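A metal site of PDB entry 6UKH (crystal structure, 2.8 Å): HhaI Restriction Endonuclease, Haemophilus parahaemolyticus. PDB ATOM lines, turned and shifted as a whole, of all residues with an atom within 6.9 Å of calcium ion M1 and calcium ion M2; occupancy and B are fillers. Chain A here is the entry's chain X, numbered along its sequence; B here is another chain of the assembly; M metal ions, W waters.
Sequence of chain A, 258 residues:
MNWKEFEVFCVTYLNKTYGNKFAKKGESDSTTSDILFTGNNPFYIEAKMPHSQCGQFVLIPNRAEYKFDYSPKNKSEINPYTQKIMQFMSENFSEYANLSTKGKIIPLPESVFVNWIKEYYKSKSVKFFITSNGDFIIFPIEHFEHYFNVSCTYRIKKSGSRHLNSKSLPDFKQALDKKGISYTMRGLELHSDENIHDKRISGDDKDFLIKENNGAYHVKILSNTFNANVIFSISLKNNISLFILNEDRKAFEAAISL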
ATOM      1  N   TRP A   3      22.660 -10.694  24.169  1.00  0.00           N
ATOM      2  CA  TRP A   3      21.439 -11.079  24.871  1.00  0.00           C
ATOM      3  C   TRP A   3      20.511 -11.882  23.972  1.00  0.00           C
ATOM      4  O   TRP A   3      19.833 -12.812  24.445  1.00  0.00           O
ATOM      5  CB  TRP A   3      20.722  -9.844  25.419  1.00  0.00           C
ATOM      6  CG  TRP A   3      20.213  -8.868  24.407  1.00  0.00           C
ATOM      7  CD1 TRP A   3      20.862  -7.764  23.941  1.00  0.00           C
ATOM      8  CD2 TRP A   3      18.926  -8.870  23.769  1.00  0.00           C
ATOM      9  NE1 TRP A   3      20.069  -7.084  23.042  1.00  0.00           N
ATOM     10  CE2 TRP A   3      18.875  -7.749  22.923  1.00  0.00           C
ATOM     11  CE3 TRP A   3      17.820  -9.726  23.823  1.00  0.00           C
ATOM     12  CZ2 TRP A   3      17.765  -7.455  22.145  1.00  0.00           C
ATOM     13  CZ3 TRP A   3      16.719  -9.432  23.049  1.00  0.00           C
ATOM     14  CH2 TRP A   3      16.694  -8.302  22.219  1.00  0.00           C
ATOM     15  N   GLU A   7      19.197 -15.447  25.248  1.00  0.00           N
ATOM     16  CA  GLU A   7      17.820 -15.909  25.394  1.00  0.00           C
ATOM     17  C   GLU A   7      17.625 -17.252  24.687  1.00  0.00           C
ATOM     18  O   GLU A   7      16.971 -18.151  25.234  1.00  0.00           O
ATOM     19  CB  GLU A   7      16.845 -14.869  24.856  1.00  0.00           C
ATOM     20  CG  GLU A   7      16.995 -13.505  25.511  1.00  0.00           C
ATOM     21  CD  GLU A   7      15.683 -12.777  25.691  1.00  0.00           C
ATOM     22  OE1 GLU A   7      15.517 -12.103  26.732  1.00  0.00           O
ATOM     23  OE2 GLU A   7      14.815 -12.860  24.785  1.00  0.00           O
ATOM     24  N   GLY A  26       9.146 -12.865  20.579  1.00  0.00           N
ATOM     25  CA  GLY A  26      10.014 -12.135  19.659  1.00  0.00           C
ATOM     26  C   GLY A  26      11.179 -11.461  20.372  1.00  0.00           C
ATOM     27  O   GLY A  26      11.065 -11.002  21.514  1.00  0.00           O
ATOM     28  N   SER A  28      13.432  -8.343  20.922  1.00  0.00           N
ATOM     29  CA  SER A  28      13.066  -6.929  20.973  1.00  0.00           C
ATOM     30  C   SER A  28      11.561  -6.732  21.047  1.00  0.00           C
ATOM     31  O   SER A  28      11.092  -5.582  21.076  1.00  0.00           O
ATOM     32  CB  SER A  28      13.625  -6.113  19.794  1.00  0.00           C
ATOM     33  OG  SER A  28      14.877  -5.540  20.128  1.00  0.00           O
ATOM     34  N   ASP A  29      10.780  -7.821  21.052  1.00  0.00           N
ATOM     35  CA  ASP A  29       9.354  -7.771  21.318  1.00  0.00           C
ATOM     36  C   ASP A  29       9.122  -7.543  22.804  1.00  0.00           C
ATOM     37  O   ASP A  29       9.557  -8.357  23.637  1.00  0.00           O
ATOM     38  CB  ASP A  29       8.724  -9.086  20.842  1.00  0.00           C
ATOM     39  CG  ASP A  29       7.242  -9.147  21.066  1.00  0.00           C
ATOM     40  OD1 ASP A  29       6.468  -8.875  20.117  1.00  0.00           O
ATOM     41  OD2 ASP A  29       6.848  -9.488  22.203  1.00  0.00           O
ATOM     42  N   SER A  30       8.458  -6.435  23.140  1.00  0.00           N
ATOM     43  CA  SER A  30       8.344  -5.983  24.529  1.00  0.00           C
ATOM     44  C   SER A  30       6.956  -6.171  25.126  1.00  0.00           C
ATOM     45  O   SER A  30       6.764  -5.903  26.314  1.00  0.00           O
ATOM     46  CB  SER A  30       8.744  -4.505  24.650  1.00  0.00           C
ATOM     47  OG  SER A  30       7.636  -3.649  24.436  1.00  0.00           O
ATOM     48  N   THR A  32       5.338  -8.717  26.018  1.00  0.00           N
ATOM     49  CA  THR A  32       5.288  -9.727  27.060  1.00  0.00           C
ATOM     50  C   THR A  32       6.706 -10.194  27.365  1.00  0.00           C
ATOM     51  O   THR A  32       7.684  -9.712  26.782  1.00  0.00           O
ATOM     52  CB  THR A  32       4.395 -10.911  26.644  1.00  0.00           C
ATOM     53  OG1 THR A  32       4.217 -11.784  27.760  1.00  0.00           O
ATOM     54  CG2 THR A  32       5.043 -11.687  25.503  1.00  0.00           C
ATOM     55  N   SER A  33       6.822 -11.125  28.306  1.00  0.00           N
ATOM     56  CA  SER A  33       8.114 -11.650  28.716  1.00  0.00           C
ATOM     57  C   SER A  33       8.629 -12.664  27.683  1.00  0.00           C
ATOM     58  O   SER A  33       7.951 -13.027  26.721  1.00  0.00           O
ATOM     59  CB  SER A  33       8.025 -12.250  30.107  1.00  0.00           C
ATOM     60  N   ASP A  34       9.850 -13.164  27.915  1.00  0.00           N
ATOM     61  CA  ASP A  34      10.599 -13.837  26.867  1.00  0.00           C
ATOM     62  C   ASP A  34      10.057 -15.224  26.553  1.00  0.00           C
ATOM     63  O   ASP A  34       9.718 -15.539  25.409  1.00  0.00           O
ATOM     64  CB  ASP A  34      12.078 -13.927  27.265  1.00  0.00           C
ATOM     65  CG  ASP A  34      12.604 -12.650  27.844  1.00  0.00           C
ATOM     66  OD1 ASP A  34      12.307 -11.569  27.300  1.00  0.00           O
ATOM     67  OD2 ASP A  34      13.326 -12.732  28.858  1.00  0.00           O
ATOM     68  N   ILE A  45       8.563 -17.110  31.701  1.00  0.00           N
ATOM     69  CA  ILE A  45       9.888 -17.053  32.292  1.00  0.00           C
ATOM     70  C   ILE A  45      10.647 -15.899  31.653  1.00  0.00           C
ATOM     71  O   ILE A  45      10.561 -15.690  30.432  1.00  0.00           O
ATOM     72  CB  ILE A  45      10.647 -18.382  32.082  1.00  0.00           C
ATOM     73  CG1 ILE A  45       9.865 -19.552  32.700  1.00  0.00           C
ATOM     74  CG2 ILE A  45      12.068 -18.303  32.646  1.00  0.00           C
ATOM     75  CD1 ILE A  45      10.475 -20.917  32.407  1.00  0.00           C
ATOM     76  N   GLU A  46      11.374 -15.146  32.464  1.00  0.00           N
ATOM     77  CA  GLU A  46      12.150 -13.995  32.002  1.00  0.00           C
ATOM     78  C   GLU A  46      13.635 -14.324  32.095  1.00  0.00           C
ATOM     79  O   GLU A  46      14.126 -14.689  33.171  1.00  0.00           O
ATOM     80  CB  GLU A  46      11.828 -12.747  32.827  1.00  0.00           C
ATOM     81  CG  GLU A  46      10.963 -11.740  32.093  1.00  0.00           C
ATOM     82  CD  GLU A  46      11.755 -10.852  31.164  1.00  0.00           C
ATOM     83  OE1 GLU A  46      12.993 -10.752  31.344  1.00  0.00           O
ATOM     84  OE2 GLU A  46      11.140 -10.250  30.255  1.00  0.00           O
ATOM     85  N   ALA A  47      14.348 -14.190  30.979  1.00  0.00           N
ATOM     86  CA  ALA A  47      15.774 -14.482  30.921  1.00  0.00           C
ATOM     87  C   ALA A  47      16.565 -13.189  31.041  1.00  0.00           C
ATOM     88  O   ALA A  47      16.373 -12.264  30.240  1.00  0.00           O
ATOM     89  CB  ALA A  47      16.130 -15.194  29.615  1.00  0.00           C
ATOM     90  N   LYS A  48      17.444 -13.122  32.031  1.00  0.00           N
ATOM     91  CA  LYS A  48      18.296 -11.966  32.251  1.00  0.00           C
ATOM     92  C   LYS A  48      19.752 -12.390  32.179  1.00  0.00           C
ATOM     93  O   LYS A  48      20.114 -13.489  32.614  1.00  0.00           O
ATOM     94  CB  LYS A  48      18.029 -11.300  33.606  1.00  0.00           C
ATOM     95  CG  LYS A  48      16.618 -10.774  33.802  1.00  0.00           C
ATOM     96  CD  LYS A  48      16.465  -9.395  33.174  1.00  0.00           C
ATOM     97  CE  LYS A  48      15.120  -8.787  33.552  1.00  0.00           C
ATOM     98  NZ  LYS A  48      14.964  -7.409  33.015  1.00  0.00           N
ATOM     99  N   MET A  49      20.579 -11.522  31.659  1.00  0.00           N
ATOM    100  CA  MET A  49      22.001 -11.809  31.775  1.00  0.00           C
ATOM    101  C   MET A  49      22.533 -11.288  33.100  1.00  0.00           C
ATOM    102  O   MET A  49      21.893 -10.462  33.752  1.00  0.00           O
ATOM    103  CB  MET A  49      22.758 -11.185  30.597  1.00  0.00           C
ATOM    104  CG  MET A  49      22.999 -12.193  29.494  1.00  0.00           C
ATOM    105  SD  MET A  49      24.160 -11.661  28.222  1.00  0.00           S
ATOM    106  CE  MET A  49      23.396 -10.173  27.665  1.00  0.00           C
ATOM    107  N   SER A  52      22.156  -6.940  33.736  1.00  0.00           N
ATOM    108  CA  SER A  52      21.002  -6.564  32.928  1.00  0.00           C
ATOM    109  C   SER A  52      20.363  -5.307  33.496  1.00  0.00           C
ATOM    110  O   SER A  52      20.738  -4.819  34.565  1.00  0.00           O
ATOM    111  CB  SER A  52      19.953  -7.695  32.880  1.00  0.00           C
ATOM    112  OG  SER A  52      20.546  -8.953  32.624  1.00  0.00           O
ATOM    113  N   GLN A  53      19.392  -4.790  32.760  1.00  0.00           N
ATOM    114  CA  GLN A  53      18.486  -3.772  33.253  1.00  0.00           C
ATOM    115  C   GLN A  53      17.108  -4.400  33.440  1.00  0.00           C
ATOM    116  O   GLN A  53      16.787  -5.429  32.841  1.00  0.00           O
ATOM    117  CB  GLN A  53      18.438  -2.572  32.311  1.00  0.00           C
ATOM    118  CG  GLN A  53      19.709  -1.726  32.416  1.00  0.00           C
ATOM    119  CD  GLN A  53      19.817  -0.649  31.355  1.00  0.00           C
ATOM    120  OE1 GLN A  53      19.968   0.528  31.664  1.00  0.00           O
ATOM    121  NE2 GLN A  53      19.744  -1.049  30.084  1.00  0.00           N
ATOM    122  N   TYR A 121       7.145  -7.600  37.284  1.00  0.00           N
ATOM    123  CA  TYR A 121       7.221  -8.867  36.564  1.00  0.00           C
ATOM    124  C   TYR A 121       6.107  -9.825  36.947  1.00  0.00           C
ATOM    125  O   TYR A 121       5.804 -10.733  36.158  1.00  0.00           O
ATOM    126  CB  TYR A 121       8.598  -9.499  36.764  1.00  0.00           C
ATOM    127  CG  TYR A 121       9.621  -8.896  35.841  1.00  0.00           C
ATOM    128  CD1 TYR A 121       9.572  -9.147  34.471  1.00  0.00           C
ATOM    129  CD2 TYR A 121      10.595  -8.029  36.317  1.00  0.00           C
ATOM    130  CE1 TYR A 121      10.483  -8.574  33.616  1.00  0.00           C
ATOM    131  CE2 TYR A 121      11.518  -7.449  35.458  1.00  0.00           C
ATOM    132  CZ  TYR A 121      11.451  -7.732  34.109  1.00  0.00           C
ATOM    133  OH  TYR A 121      12.364  -7.153  33.247  1.00  0.00           O
ATOM    134  P    DG B   8      10.047  -3.383  29.734  1.00  0.00           P
ATOM    135  OP1  DG B   8       9.281  -4.514  30.282  1.00  0.00           O
ATOM    136  OP2  DG B   8      10.863  -2.532  30.643  1.00  0.00           O
ATOM    137  O5'  DG B   8      10.993  -3.970  28.588  1.00  0.00           O
ATOM    138  C5'  DG B   8      10.562  -5.089  27.837  1.00  0.00           C
ATOM    139  C4'  DG B   8      11.596  -5.465  26.783  1.00  0.00           C
ATOM    140  O4'  DG B   8      11.751  -4.366  25.877  1.00  0.00           O
ATOM    141  C3'  DG B   8      12.979  -5.759  27.331  1.00  0.00           C
ATOM    142  O3'  DG B   8      13.103  -7.165  27.568  1.00  0.00           O
ATOM    143  C2'  DG B   8      13.893  -5.333  26.201  1.00  0.00           C
ATOM    144  C1'  DG B   8      13.114  -4.240  25.487  1.00  0.00           C
ATOM    145  N9   DG B   8      13.563  -2.887  25.793  1.00  0.00           N
ATOM    146  C8   DG B   8      13.148  -2.097  26.832  1.00  0.00           C
ATOM    147  N7   DG B   8      13.716  -0.920  26.844  1.00  0.00           N
ATOM    148  C5   DG B   8      14.551  -0.934  25.724  1.00  0.00           C
ATOM    149  C6   DG B   8      15.423   0.063  25.216  1.00  0.00           C
ATOM    150  O6   DG B   8      15.630   1.202  25.660  1.00  0.00           O
ATOM    151  N1   DG B   8      16.076  -0.371  24.068  1.00  0.00           N
ATOM    152  C2   DG B   8      15.936  -1.597  23.487  1.00  0.00           C
ATOM    153  N2   DG B   8      16.655  -1.827  22.378  1.00  0.00           N
ATOM    154  N3   DG B   8      15.124  -2.546  23.949  1.00  0.00           N
ATOM    155  C4   DG B   8      14.471  -2.144  25.072  1.00  0.00           C
ATOM    156  P    DC B   9      14.189  -7.758  28.591  1.00  0.00           P
ATOM    157  OP1  DC B   9      13.958  -9.208  28.503  1.00  0.00           O
ATOM    158  OP2  DC B   9      14.098  -7.074  29.906  1.00  0.00           O
ATOM    159  O5'  DC B   9      15.606  -7.386  27.938  1.00  0.00           O
ATOM    160  C5'  DC B   9      15.972  -7.942  26.681  1.00  0.00           C
ATOM    161  C4'  DC B   9      17.202  -7.256  26.126  1.00  0.00           C
ATOM    162  O4'  DC B   9      16.860  -5.960  25.575  1.00  0.00           O
ATOM    163  C3'  DC B   9      18.269  -6.927  27.141  1.00  0.00           C
ATOM    164  O3'  DC B   9      19.022  -8.074  27.484  1.00  0.00           O
ATOM    165  C2'  DC B   9      19.100  -5.913  26.353  1.00  0.00           C
ATOM    166  C1'  DC B   9      17.999  -5.113  25.658  1.00  0.00           C
ATOM    167  N1   DC B   9      17.635  -3.869  26.399  1.00  0.00           N
ATOM    168  C2   DC B   9      18.234  -2.638  26.053  1.00  0.00           C
ATOM    169  O2   DC B   9      19.022  -2.611  25.107  1.00  0.00           O
ATOM    170  N3   DC B   9      17.909  -1.522  26.760  1.00  0.00           N
ATOM    171  C4   DC B   9      17.041  -1.608  27.776  1.00  0.00           C
ATOM    172  N4   DC B   9      16.743  -0.492  28.440  1.00  0.00           N
ATOM    173  C5   DC B   9      16.432  -2.848  28.150  1.00  0.00           C
ATOM    174  C6   DC B   9      16.753  -3.935  27.452  1.00  0.00           C
ATOM    175  P    DT B  10      19.282  -8.383  29.036  1.00  0.00           P
ATOM    176  OP1  DT B  10      19.844  -9.741  29.168  1.00  0.00           O
ATOM    177  OP2  DT B  10      18.013  -8.045  29.733  1.00  0.00           O
ATOM    178  O5'  DT B  10      20.393  -7.303  29.478  1.00  0.00           O
ATOM    179  C5'  DT B  10      21.760  -7.487  29.124  1.00  0.00           C
ATOM    180  C4'  DT B  10      22.137  -6.608  27.941  1.00  0.00           C
ATOM    181  O4'  DT B  10      21.965  -5.206  28.293  1.00  0.00           O
ATOM    182  C3'  DT B  10      23.592  -6.747  27.469  1.00  0.00           C
ATOM    183  O3'  DT B  10      23.643  -6.645  26.043  1.00  0.00           O
ATOM    184  C2'  DT B  10      24.275  -5.554  28.147  1.00  0.00           C
ATOM    185  C1'  DT B  10      23.172  -4.506  28.073  1.00  0.00           C
ATOM    186  N1   DT B  10      23.287  -3.413  29.111  1.00  0.00           N
ATOM    187  C2   DT B  10      23.322  -2.096  28.690  1.00  0.00           C
ATOM    188  O2   DT B  10      23.263  -1.757  27.529  1.00  0.00           O
ATOM    189  N3   DT B  10      23.401  -1.177  29.696  1.00  0.00           N
ATOM    190  C4   DT B  10      23.466  -1.437  31.055  1.00  0.00           C
ATOM    191  O4   DT B  10      23.551  -0.531  31.881  1.00  0.00           O
ATOM    192  C5   DT B  10      23.433  -2.840  31.421  1.00  0.00           C
ATOM    193  C7   DT B  10      23.489  -3.250  32.870  1.00  0.00           C
ATOM    194  C6   DT B  10      23.333  -3.747  30.444  1.00  0.00           C
HETATM  195 CA    CA M   1      14.824 -10.851  29.386  1.00  0.00          CA
HETATM  196 CA    CA M   2      11.876  -9.316  26.914  1.00  0.00          CA
HETATM  197  O   HOH W   1      13.562 -10.205  25.101  1.00  0.00           O
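N4 of DC 9 of chain B lies within hydrogen-bond range of NE2 of Gln 53.
OP2 of DC 9 of chain B is in salt-bridge range of NZ of Lys 48, 3.2 Å away.
Within 4 Å of calcium ion M1: Glu 7, Asp 34, Glu 46, Ala 47 and DC 9 of chain B.
Calcium ion M1 is bound by OP1 of DC 9 of chain B (2.1 Å), the backbone carbonyl oxygen of Ala 47 (2.3 Å), the side-chain carboxylate of Asp 34 (2.5 Å) and the side-chain carboxylate of Glu 46 (2.7 Å).
Calcium ion M1 has four donor atoms within binding distance.
Slightly farther from calcium ion M1 lies OE1 of Glu 7 (3.0 Å).
Calcium ion M2 is bound by the side-chain carboxylate (OD1) of Asp 34, O3' of DG 8 of chain B, OP1 of DC 9 of chain B and water W1.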
